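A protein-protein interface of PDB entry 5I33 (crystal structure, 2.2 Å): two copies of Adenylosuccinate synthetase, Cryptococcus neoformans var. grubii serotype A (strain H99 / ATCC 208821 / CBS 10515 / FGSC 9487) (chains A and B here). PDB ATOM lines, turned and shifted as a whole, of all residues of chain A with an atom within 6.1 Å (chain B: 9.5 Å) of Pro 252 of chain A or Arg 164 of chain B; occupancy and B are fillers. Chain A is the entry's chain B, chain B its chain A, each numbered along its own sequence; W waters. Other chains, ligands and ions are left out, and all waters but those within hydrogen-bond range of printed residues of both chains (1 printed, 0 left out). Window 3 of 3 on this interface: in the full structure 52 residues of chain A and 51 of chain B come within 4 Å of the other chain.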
ATOM      1  N   GLY A 155      20.439 -11.172 -14.887  1.00  0.00           N
ATOM      2  CA  GLY A 155      19.190 -11.219 -15.627  1.00  0.00           C
ATOM      3  C   GLY A 155      18.291 -12.370 -15.193  1.00  0.00           C
ATOM      4  O   GLY A 155      17.134 -12.157 -14.825  1.00  0.00           O
ATOM      5  N   LEU A 246      16.427  -0.617 -17.630  1.00  0.00           N
ATOM      6  CA  LEU A 246      15.542  -1.638 -18.194  1.00  0.00           C
ATOM      7  C   LEU A 246      14.374  -1.007 -18.945  1.00  0.00           C
ATOM      8  O   LEU A 246      13.984  -1.491 -19.996  1.00  0.00           O
ATOM      9  CB  LEU A 246      15.006  -2.584 -17.084  1.00  0.00           C
ATOM     10  CG  LEU A 246      14.095  -3.720 -17.591  1.00  0.00           C
ATOM     11  CD1 LEU A 246      14.795  -4.437 -18.756  1.00  0.00           C
ATOM     12  CD2 LEU A 246      13.692  -4.703 -16.493  1.00  0.00           C
ATOM     13  N   THR A 250      18.487   1.842 -24.191  1.00  0.00           N
ATOM     14  CA  THR A 250      18.418   1.347 -25.561  1.00  0.00           C
ATOM     15  C   THR A 250      18.023  -0.134 -25.583  1.00  0.00           C
ATOM     16  O   THR A 250      18.807  -0.989 -26.008  1.00  0.00           O
ATOM     17  CB  THR A 250      19.767   1.558 -26.316  1.00  0.00           C
ATOM     18  OG1 THR A 250      20.868   1.057 -25.546  1.00  0.00           O
ATOM     19  CG2 THR A 250      19.987   3.038 -26.596  1.00  0.00           C
ATOM     20  N   TYR A 251      16.828  -0.433 -25.070  1.00  0.00           N
ATOM     21  CA  TYR A 251      16.297  -1.798 -25.055  1.00  0.00           C
ATOM     22  C   TYR A 251      16.350  -2.371 -26.466  1.00  0.00           C
ATOM     23  O   TYR A 251      16.023  -1.661 -27.407  1.00  0.00           O
ATOM     24  CB  TYR A 251      14.855  -1.806 -24.523  1.00  0.00           C
ATOM     25  CG  TYR A 251      14.233  -3.173 -24.334  1.00  0.00           C
ATOM     26  CD1 TYR A 251      13.767  -3.917 -25.419  1.00  0.00           C
ATOM     27  CD2 TYR A 251      14.069  -3.708 -23.054  1.00  0.00           C
ATOM     28  CE1 TYR A 251      13.194  -5.163 -25.239  1.00  0.00           C
ATOM     29  CE2 TYR A 251      13.476  -4.953 -22.867  1.00  0.00           C
ATOM     30  CZ  TYR A 251      13.043  -5.671 -23.949  1.00  0.00           C
ATOM     31  OH  TYR A 251      12.459  -6.912 -23.764  1.00  0.00           O
ATOM     32  N   PRO A 252      16.749  -3.653 -26.621  1.00  0.00           N
ATOM     33  CA  PRO A 252      17.103  -4.623 -25.571  1.00  0.00           C
ATOM     34  C   PRO A 252      18.559  -4.567 -25.072  1.00  0.00           C
ATOM     35  O   PRO A 252      18.949  -5.403 -24.259  1.00  0.00           O
ATOM     36  CB  PRO A 252      16.815  -5.971 -26.245  1.00  0.00           C
ATOM     37  CG  PRO A 252      17.135  -5.720 -27.691  1.00  0.00           C
ATOM     38  CD  PRO A 252      16.701  -4.290 -27.955  1.00  0.00           C
ATOM     39  N   PHE A 253      19.334  -3.592 -25.529  1.00  0.00           N
ATOM     40  CA  PHE A 253      20.719  -3.454 -25.096  1.00  0.00           C
ATOM     41  C   PHE A 253      20.787  -2.658 -23.800  1.00  0.00           C
ATOM     42  O   PHE A 253      21.299  -1.530 -23.767  1.00  0.00           O
ATOM     43  CB  PHE A 253      21.562  -2.788 -26.195  1.00  0.00           C
ATOM     44  CG  PHE A 253      21.472  -3.486 -27.515  1.00  0.00           C
ATOM     45  CD1 PHE A 253      22.201  -4.632 -27.758  1.00  0.00           C
ATOM     46  CD2 PHE A 253      20.619  -3.024 -28.499  1.00  0.00           C
ATOM     47  CE1 PHE A 253      22.107  -5.286 -28.973  1.00  0.00           C
ATOM     48  CE2 PHE A 253      20.521  -3.674 -29.713  1.00  0.00           C
ATOM     49  CZ  PHE A 253      21.264  -4.804 -29.947  1.00  0.00           C
ATOM     50  N   VAL A 254      20.236  -3.250 -22.736  1.00  0.00           N
ATOM     51  CA  VAL A 254      20.182  -2.620 -21.420  1.00  0.00           C
ATOM     52  C   VAL A 254      20.421  -3.682 -20.342  1.00  0.00           C
ATOM     53  O   VAL A 254      20.549  -4.863 -20.671  1.00  0.00           O
ATOM     54  CB  VAL A 254      18.818  -1.935 -21.181  1.00  0.00           C
ATOM     55  CG1 VAL A 254      18.559  -0.864 -22.231  1.00  0.00           C
ATOM     56  CG2 VAL A 254      17.673  -2.982 -21.157  1.00  0.00           C
ATOM     57  N   THR A 255      20.487  -3.281 -19.068  1.00  0.00           N
ATOM     58  CA  THR A 255      20.541  -4.271 -17.989  1.00  0.00           C
ATOM     59  C   THR A 255      19.123  -4.714 -17.611  1.00  0.00           C
ATOM     60  O   THR A 255      18.130  -4.208 -18.155  1.00  0.00           O
ATOM     61  CB  THR A 255      21.274  -3.753 -16.712  1.00  0.00           C
ATOM     62  OG1 THR A 255      20.569  -2.635 -16.158  1.00  0.00           O
ATOM     63  CG2 THR A 255      22.705  -3.340 -17.038  1.00  0.00           C
ATOM     64  N   SER A 256      19.026  -5.645 -16.664  1.00  0.00           N
ATOM     65  CA  SER A 256      17.759  -6.279 -16.389  1.00  0.00           C
ATOM     66  C   SER A 256      17.022  -5.639 -15.217  1.00  0.00           C
ATOM     67  O   SER A 256      16.118  -6.242 -14.648  1.00  0.00           O
ATOM     68  CB  SER A 256      17.978  -7.769 -16.135  1.00  0.00           C
ATOM     69  OG  SER A 256      19.012  -7.990 -15.192  1.00  0.00           O
ATOM     70  N   LEU A 377      15.024   1.231 -32.237  1.00  0.00           N
ATOM     71  CA  LEU A 377      16.454   1.302 -32.494  1.00  0.00           C
ATOM     72  C   LEU A 377      16.776   1.457 -33.988  1.00  0.00           C
ATOM     73  O   LEU A 377      17.835   1.959 -34.329  1.00  0.00           O
ATOM     74  CB  LEU A 377      17.156   0.072 -31.912  1.00  0.00           C
ATOM     75  CG  LEU A 377      17.153   0.009 -30.380  1.00  0.00           C
ATOM     76  CD1 LEU A 377      17.917  -1.207 -29.883  1.00  0.00           C
ATOM     77  CD2 LEU A 377      17.714   1.292 -29.776  1.00  0.00           C
ATOM     78  N   HIS B 125       5.493  -2.861 -22.225  1.00  0.00           N
ATOM     79  CA  HIS B 125       5.660  -4.215 -22.751  1.00  0.00           C
ATOM     80  C   HIS B 125       4.337  -4.856 -23.147  1.00  0.00           C
ATOM     81  O   HIS B 125       3.271  -4.387 -22.757  1.00  0.00           O
ATOM     82  CB  HIS B 125       6.413  -5.085 -21.762  1.00  0.00           C
ATOM     83  CG  HIS B 125       7.891  -4.883 -21.824  1.00  0.00           C
ATOM     84  ND1 HIS B 125       8.753  -5.839 -22.318  1.00  0.00           N
ATOM     85  CD2 HIS B 125       8.657  -3.820 -21.489  1.00  0.00           C
ATOM     86  CE1 HIS B 125       9.988  -5.380 -22.271  1.00  0.00           C
ATOM     87  NE2 HIS B 125       9.957  -4.157 -21.774  1.00  0.00           N
ATOM     88  N   PRO B 156       4.447 -13.725 -16.395  1.00  0.00           N
ATOM     89  CA  PRO B 156       5.305 -14.147 -17.513  1.00  0.00           C
ATOM     90  C   PRO B 156       5.782 -12.988 -18.406  1.00  0.00           C
ATOM     91  O   PRO B 156       6.910 -13.010 -18.884  1.00  0.00           O
ATOM     92  CB  PRO B 156       4.404 -15.111 -18.283  1.00  0.00           C
ATOM     93  CG  PRO B 156       3.557 -15.754 -17.163  1.00  0.00           C
ATOM     94  CD  PRO B 156       3.288 -14.623 -16.207  1.00  0.00           C
ATOM     95  N   ALA B 157       4.936 -11.984 -18.604  1.00  0.00           N
ATOM     96  CA  ALA B 157       5.318 -10.815 -19.374  1.00  0.00           C
ATOM     97  C   ALA B 157       6.396 -10.006 -18.647  1.00  0.00           C
ATOM     98  O   ALA B 157       7.348  -9.540 -19.271  1.00  0.00           O
ATOM     99  CB  ALA B 157       4.098  -9.965 -19.671  1.00  0.00           C
ATOM    100  N   TYR B 158       6.259  -9.828 -17.331  1.00  0.00           N
ATOM    101  CA  TYR B 158       7.314  -9.151 -16.584  1.00  0.00           C
ATOM    102  C   TYR B 158       8.595  -9.976 -16.542  1.00  0.00           C
ATOM    103  O   TYR B 158       9.683  -9.441 -16.407  1.00  0.00           O
ATOM    104  CB  TYR B 158       6.866  -8.822 -15.174  1.00  0.00           C
ATOM    105  CG  TYR B 158       6.124  -7.521 -15.120  1.00  0.00           C
ATOM    106  CD1 TYR B 158       6.764  -6.323 -15.439  1.00  0.00           C
ATOM    107  CD2 TYR B 158       4.785  -7.478 -14.752  1.00  0.00           C
ATOM    108  CE1 TYR B 158       6.082  -5.121 -15.389  1.00  0.00           C
ATOM    109  CE2 TYR B 158       4.098  -6.290 -14.704  1.00  0.00           C
ATOM    110  CZ  TYR B 158       4.750  -5.111 -15.014  1.00  0.00           C
ATOM    111  OH  TYR B 158       4.043  -3.933 -14.954  1.00  0.00           O
ATOM    112  N   SER B 159       8.462 -11.286 -16.650  1.00  0.00           N
ATOM    113  CA  SER B 159       9.622 -12.166 -16.723  1.00  0.00           C
ATOM    114  C   SER B 159      10.402 -11.984 -18.036  1.00  0.00           C
ATOM    115  O   SER B 159      11.631 -11.984 -18.040  1.00  0.00           O
ATOM    116  CB  SER B 159       9.183 -13.620 -16.550  1.00  0.00           C
ATOM    117  OG  SER B 159      10.305 -14.472 -16.556  1.00  0.00           O
ATOM    118  N   SER B 160       9.681 -11.890 -19.151  1.00  0.00           N
ATOM    119  CA  SER B 160      10.294 -11.618 -20.456  1.00  0.00           C
ATOM    120  C   SER B 160      10.977 -10.257 -20.471  1.00  0.00           C
ATOM    121  O   SER B 160      12.016 -10.088 -21.102  1.00  0.00           O
ATOM    122  CB  SER B 160       9.256 -11.669 -21.572  1.00  0.00           C
ATOM    123  OG  SER B 160       8.738 -12.979 -21.719  1.00  0.00           O
ATOM    124  N   LYS B 161      10.380  -9.290 -19.776  1.00  0.00           N
ATOM    125  CA  LYS B 161      10.922  -7.947 -19.714  1.00  0.00           C
ATOM    126  C   LYS B 161      12.307  -7.990 -19.090  1.00  0.00           C
ATOM    127  O   LYS B 161      13.268  -7.418 -19.635  1.00  0.00           O
ATOM    128  CB  LYS B 161       9.993  -7.023 -18.921  1.00  0.00           C
ATOM    129  CG  LYS B 161      10.463  -5.571 -18.777  1.00  0.00           C
ATOM    130  CD  LYS B 161       9.423  -4.730 -18.033  1.00  0.00           C
ATOM    131  CE  LYS B 161       9.828  -3.267 -17.944  1.00  0.00           C
ATOM    132  NZ  LYS B 161       8.736  -2.473 -17.283  1.00  0.00           N
ATOM    133  N   ALA B 162      12.404  -8.662 -17.942  1.00  0.00           N
ATOM    134  CA  ALA B 162      13.675  -8.816 -17.229  1.00  0.00           C
ATOM    135  C   ALA B 162      14.726  -9.574 -18.062  1.00  0.00           C
ATOM    136  O   ALA B 162      15.936  -9.354 -17.913  1.00  0.00           O
ATOM    137  CB  ALA B 162      13.444  -9.523 -15.888  1.00  0.00           C
ATOM    138  N   SER B 163      14.254 -10.499 -18.898  1.00  0.00           N
ATOM    139  CA  SER B 163      15.118 -11.260 -19.794  1.00  0.00           C
ATOM    140  C   SER B 163      15.511 -10.415 -21.013  1.00  0.00           C
ATOM    141  O   SER B 163      16.423 -10.774 -21.774  1.00  0.00           O
ATOM    142  CB  SER B 163      14.424 -12.550 -20.250  1.00  0.00           C
ATOM    143  OG  SER B 163      14.227 -13.432 -19.159  1.00  0.00           O
ATOM    144  N   ARG B 164      14.775  -9.321 -21.209  1.00  0.00           N
ATOM    145  CA  ARG B 164      14.984  -8.399 -22.322  1.00  0.00           C
ATOM    146  C   ARG B 164      14.730  -9.120 -23.648  1.00  0.00           C
ATOM    147  O   ARG B 164      15.253  -8.741 -24.689  1.00  0.00           O
ATOM    148  CB  ARG B 164      16.388  -7.781 -22.240  1.00  0.00           C
ATOM    149  CG  ARG B 164      16.627  -7.209 -20.834  1.00  0.00           C
ATOM    150  CD  ARG B 164      17.961  -6.531 -20.616  1.00  0.00           C
ATOM    151  NE  ARG B 164      19.150  -7.323 -20.937  1.00  0.00           N
ATOM    152  CZ  ARG B 164      19.610  -8.332 -20.206  1.00  0.00           C
ATOM    153  NH1 ARG B 164      18.965  -8.714 -19.111  1.00  0.00           N
ATOM    154  NH2 ARG B 164      20.712  -8.972 -20.575  1.00  0.00           N
ATOM    155  N   SER B 165      13.897 -10.155 -23.590  1.00  0.00           N
ATOM    156  CA  SER B 165      13.421 -10.838 -24.778  1.00  0.00           C
ATOM    157  C   SER B 165      11.950 -10.517 -24.995  1.00  0.00           C
ATOM    158  O   SER B 165      11.324 -11.018 -25.928  1.00  0.00           O
ATOM    159  CB  SER B 165      13.604 -12.348 -24.658  1.00  0.00           C
ATOM    160  OG  SER B 165      12.813 -12.852 -23.601  1.00  0.00           O
ATOM    161  N   GLY B 166      11.391  -9.691 -24.119  1.00  0.00           N
ATOM    162  CA  GLY B 166      10.005  -9.289 -24.269  1.00  0.00           C
ATOM    163  C   GLY B 166       9.831  -8.361 -25.456  1.00  0.00           C
ATOM    164  O   GLY B 166      10.793  -7.747 -25.917  1.00  0.00           O
ATOM    165  N   LEU B 167       8.602  -8.267 -25.950  1.00  0.00           N
ATOM    166  CA  LEU B 167       8.265  -7.365 -27.039  1.00  0.00           C
ATOM    167  C   LEU B 167       7.577  -6.130 -26.461  1.00  0.00           C
ATOM    168  O   LEU B 167       6.776  -6.239 -25.524  1.00  0.00           O
ATOM    169  CB  LEU B 167       7.358  -8.060 -28.047  1.00  0.00           C
ATOM    170  CG  LEU B 167       7.999  -9.229 -28.789  1.00  0.00           C
ATOM    171  CD1 LEU B 167       6.989  -9.930 -29.686  1.00  0.00           C
ATOM    172  CD2 LEU B 167       9.179  -8.736 -29.608  1.00  0.00           C
ATOM    173  N   ARG B 168       7.887  -4.955 -27.002  1.00  0.00           N
ATOM    174  CA  ARG B 168       7.319  -3.713 -26.479  1.00  0.00           C
ATOM    175  C   ARG B 168       6.369  -3.122 -27.510  1.00  0.00           C
ATOM    176  O   ARG B 168       6.267  -3.645 -28.623  1.00  0.00           O
ATOM    177  CB  ARG B 168       8.421  -2.726 -26.086  1.00  0.00           C
ATOM    178  CG  ARG B 168       9.525  -3.385 -25.277  1.00  0.00           C
ATOM    179  CD  ARG B 168      10.326  -2.368 -24.493  1.00  0.00           C
ATOM    180  NE  ARG B 168      10.988  -1.445 -25.397  1.00  0.00           N
ATOM    181  CZ  ARG B 168      11.771  -0.443 -25.019  1.00  0.00           C
ATOM    182  NH1 ARG B 168      12.007  -0.241 -23.737  1.00  0.00           N
ATOM    183  NH2 ARG B 168      12.335   0.342 -25.941  1.00  0.00           N
ATOM    184  N   HIS B 170       6.428  -0.529 -29.384  1.00  0.00           N
ATOM    185  CA  HIS B 170       7.048  -0.076 -30.656  1.00  0.00           C
ATOM    186  C   HIS B 170       7.338  -1.241 -31.598  1.00  0.00           C
ATOM    187  O   HIS B 170       7.406  -1.052 -32.810  1.00  0.00           O
ATOM    188  CB  HIS B 170       8.331   0.745 -30.408  1.00  0.00           C
ATOM    189  CG  HIS B 170       9.424  -0.006 -29.708  1.00  0.00           C
ATOM    190  ND1 HIS B 170      10.324  -0.813 -30.375  1.00  0.00           N
ATOM    191  CD2 HIS B 170       9.748  -0.088 -28.393  1.00  0.00           C
ATOM    192  CE1 HIS B 170      11.159  -1.351 -29.503  1.00  0.00           C
ATOM    193  NE2 HIS B 170      10.829  -0.929 -28.294  1.00  0.00           N
ATOM    194  N   HIS B 171       7.481  -2.448 -31.054  1.00  0.00           N
ATOM    195  CA  HIS B 171       7.738  -3.616 -31.890  1.00  0.00           C
ATOM    196  C   HIS B 171       6.591  -3.950 -32.838  1.00  0.00           C
ATOM    197  O   HIS B 171       6.796  -4.629 -33.844  1.00  0.00           O
ATOM    198  CB  HIS B 171       8.055  -4.834 -31.033  1.00  0.00           C
ATOM    199  CG  HIS B 171       9.455  -4.842 -30.514  1.00  0.00           C
ATOM    200  ND1 HIS B 171       9.754  -4.837 -29.168  1.00  0.00           N
ATOM    201  CD2 HIS B 171      10.640  -4.772 -31.164  1.00  0.00           C
ATOM    202  CE1 HIS B 171      11.068  -4.813 -29.013  1.00  0.00           C
ATOM    203  NE2 HIS B 171      11.628  -4.766 -30.212  1.00  0.00           N
ATOM    204  N   ASP B 174       7.427  -2.711 -36.049  1.00  0.00           N
ATOM    205  CA  ASP B 174       8.725  -3.225 -36.463  1.00  0.00           C
ATOM    206  C   ASP B 174       8.529  -4.384 -37.451  1.00  0.00           C
ATOM    207  O   ASP B 174       7.843  -5.355 -37.139  1.00  0.00           O
ATOM    208  CB  ASP B 174       9.498  -3.643 -35.205  1.00  0.00           C
ATOM    209  CG  ASP B 174      10.882  -4.187 -35.487  1.00  0.00           C
ATOM    210  OD1 ASP B 174      11.123  -4.745 -36.572  1.00  0.00           O
ATOM    211  OD2 ASP B 174      11.740  -4.047 -34.587  1.00  0.00           O
ATOM    212  N   LYS B 180      10.908 -12.367 -34.644  1.00  0.00           N
ATOM    213  CA  LYS B 180      11.318 -12.539 -33.253  1.00  0.00           C
ATOM    214  C   LYS B 180      10.157 -12.953 -32.346  1.00  0.00           C
ATOM    215  O   LYS B 180      10.339 -13.182 -31.147  1.00  0.00           O
ATOM    216  CB  LYS B 180      11.969 -11.267 -32.712  1.00  0.00           C
ATOM    217  CG  LYS B 180      11.090 -10.037 -32.734  1.00  0.00           C
ATOM    218  CD  LYS B 180      11.910  -8.810 -32.379  1.00  0.00           C
ATOM    219  CE  LYS B 180      13.098  -8.666 -33.309  1.00  0.00           C
ATOM    220  NZ  LYS B 180      13.686  -7.309 -33.222  1.00  0.00           N
HETATM  221  O   HOH W   1      14.270  -2.819 -29.589  1.00  0.00           O
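Of the printed residues of chain B, Tyr 251 of chain A touches His 125, Arg 164, Ser 165, Gly 166 and Arg 168.
Pro 252 of chain A touches just one residue of chain B: Arg 164.
Of chain B, only Arg 164 (2.8 Å) comes within 4 Å of Val 254 of chain A.
Of the printed residues of chain A, Ala 162 of chain B touches Ser 256.
Arg 164 of chain B touches six residues of chain A.
Printed residues of chain A within 4 Å of Ser 165 of chain B: Tyr 251 (3.6 Å).
Printed residues of chain A within 4 Å of Arg 168 of chain B: Tyr 251.
The nearest residue of chain B that does not touch Pro 252 of chain A is His 171 of chain B (5.6 Å).
The backbone NH (N) of Ser 165 of chain B sits at hydrogen-bond distance from the backbone carbonyl oxygen (O) of Ser 160 of chain B, at 3.1 Å.
The backbone carbonyl oxygen (O) of Ser 160 of chain B sits at hydrogen-bond distance from the backbone NH (N) of Gly 166 of chain B.
O of Ala 162 of chain B is in hydrogen-bond range of NH1 of Arg 164 of chain B, 3.3 Å away.
NE of Arg 168 of chain B sits at hydrogen-bond distance from NE2 of His 170 of chain B, 2.9 Å away.
The backbone NH (N) of Arg 168 of chain B is in hydrogen-bond range of a ring nitrogen (ND1) of His 171 of chain B (2.9 Å).
Leu 246 of chain A touches Lys 161 of chain B.
Leu 246 of chain A touches Arg 164 of chain B (CD1 to CG, 3.9 Å).
OH of Tyr 251 of chain A touches CE1 of His 125 of chain B, 3.3 Å away.
Ser 165 of chain B touches Tyr 251 of chain A (N to OH, 3.6 Å).
Tyr 251 of chain A touches Arg 168 of chain B (CB to NH1, 3.3 Å).
Arg 164 of chain B touches Pro 252 of chain A (O to CB, 3.5 Å).
O of Thr 255 of chain A touches CD of Arg 164 of chain B, at 3.4 Å.
O of Ala 162 of chain B touches CB of Ser 256 of chain A (3.1 Å).
NH1 of Arg 164 of chain B touches CB of Ser 256 of chain A, 3.3 Å away.
The backbone carbonyl oxygen (O) of Arg 164 of chain B sits close to the side-chain hydroxyl (OH) of Tyr 251 of chain A.
The guanidinium group (NE) of Arg 164 of chain B lies within hydrogen-bond range of the backbone carbonyl oxygen (O) of Val 254 of chain A (2.8 Å).
The backbone carbonyl oxygen of Gly 166 of chain B sits at hydrogen-bond distance from the side-chain hydroxyl of Tyr 251 of chain A (2.8 Å).
Of the 18 printed residues of chain B, 7 touch a printed residue of chain A.
Along chain B the printed residues that touch a printed residue of chain A span positions 125 to 168.
Hydrophobic or aromatic side chains of chain A that line the printed part of chain B: Leu 246, Tyr 251, Pro 252 and Val 254.
No position is printed for both chains.
Water W1 lies within hydrogen-bond range of O of Tyr 251 of chain A (3.0 Å) and NE2 of His 171 of chain B (3.3 Å).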
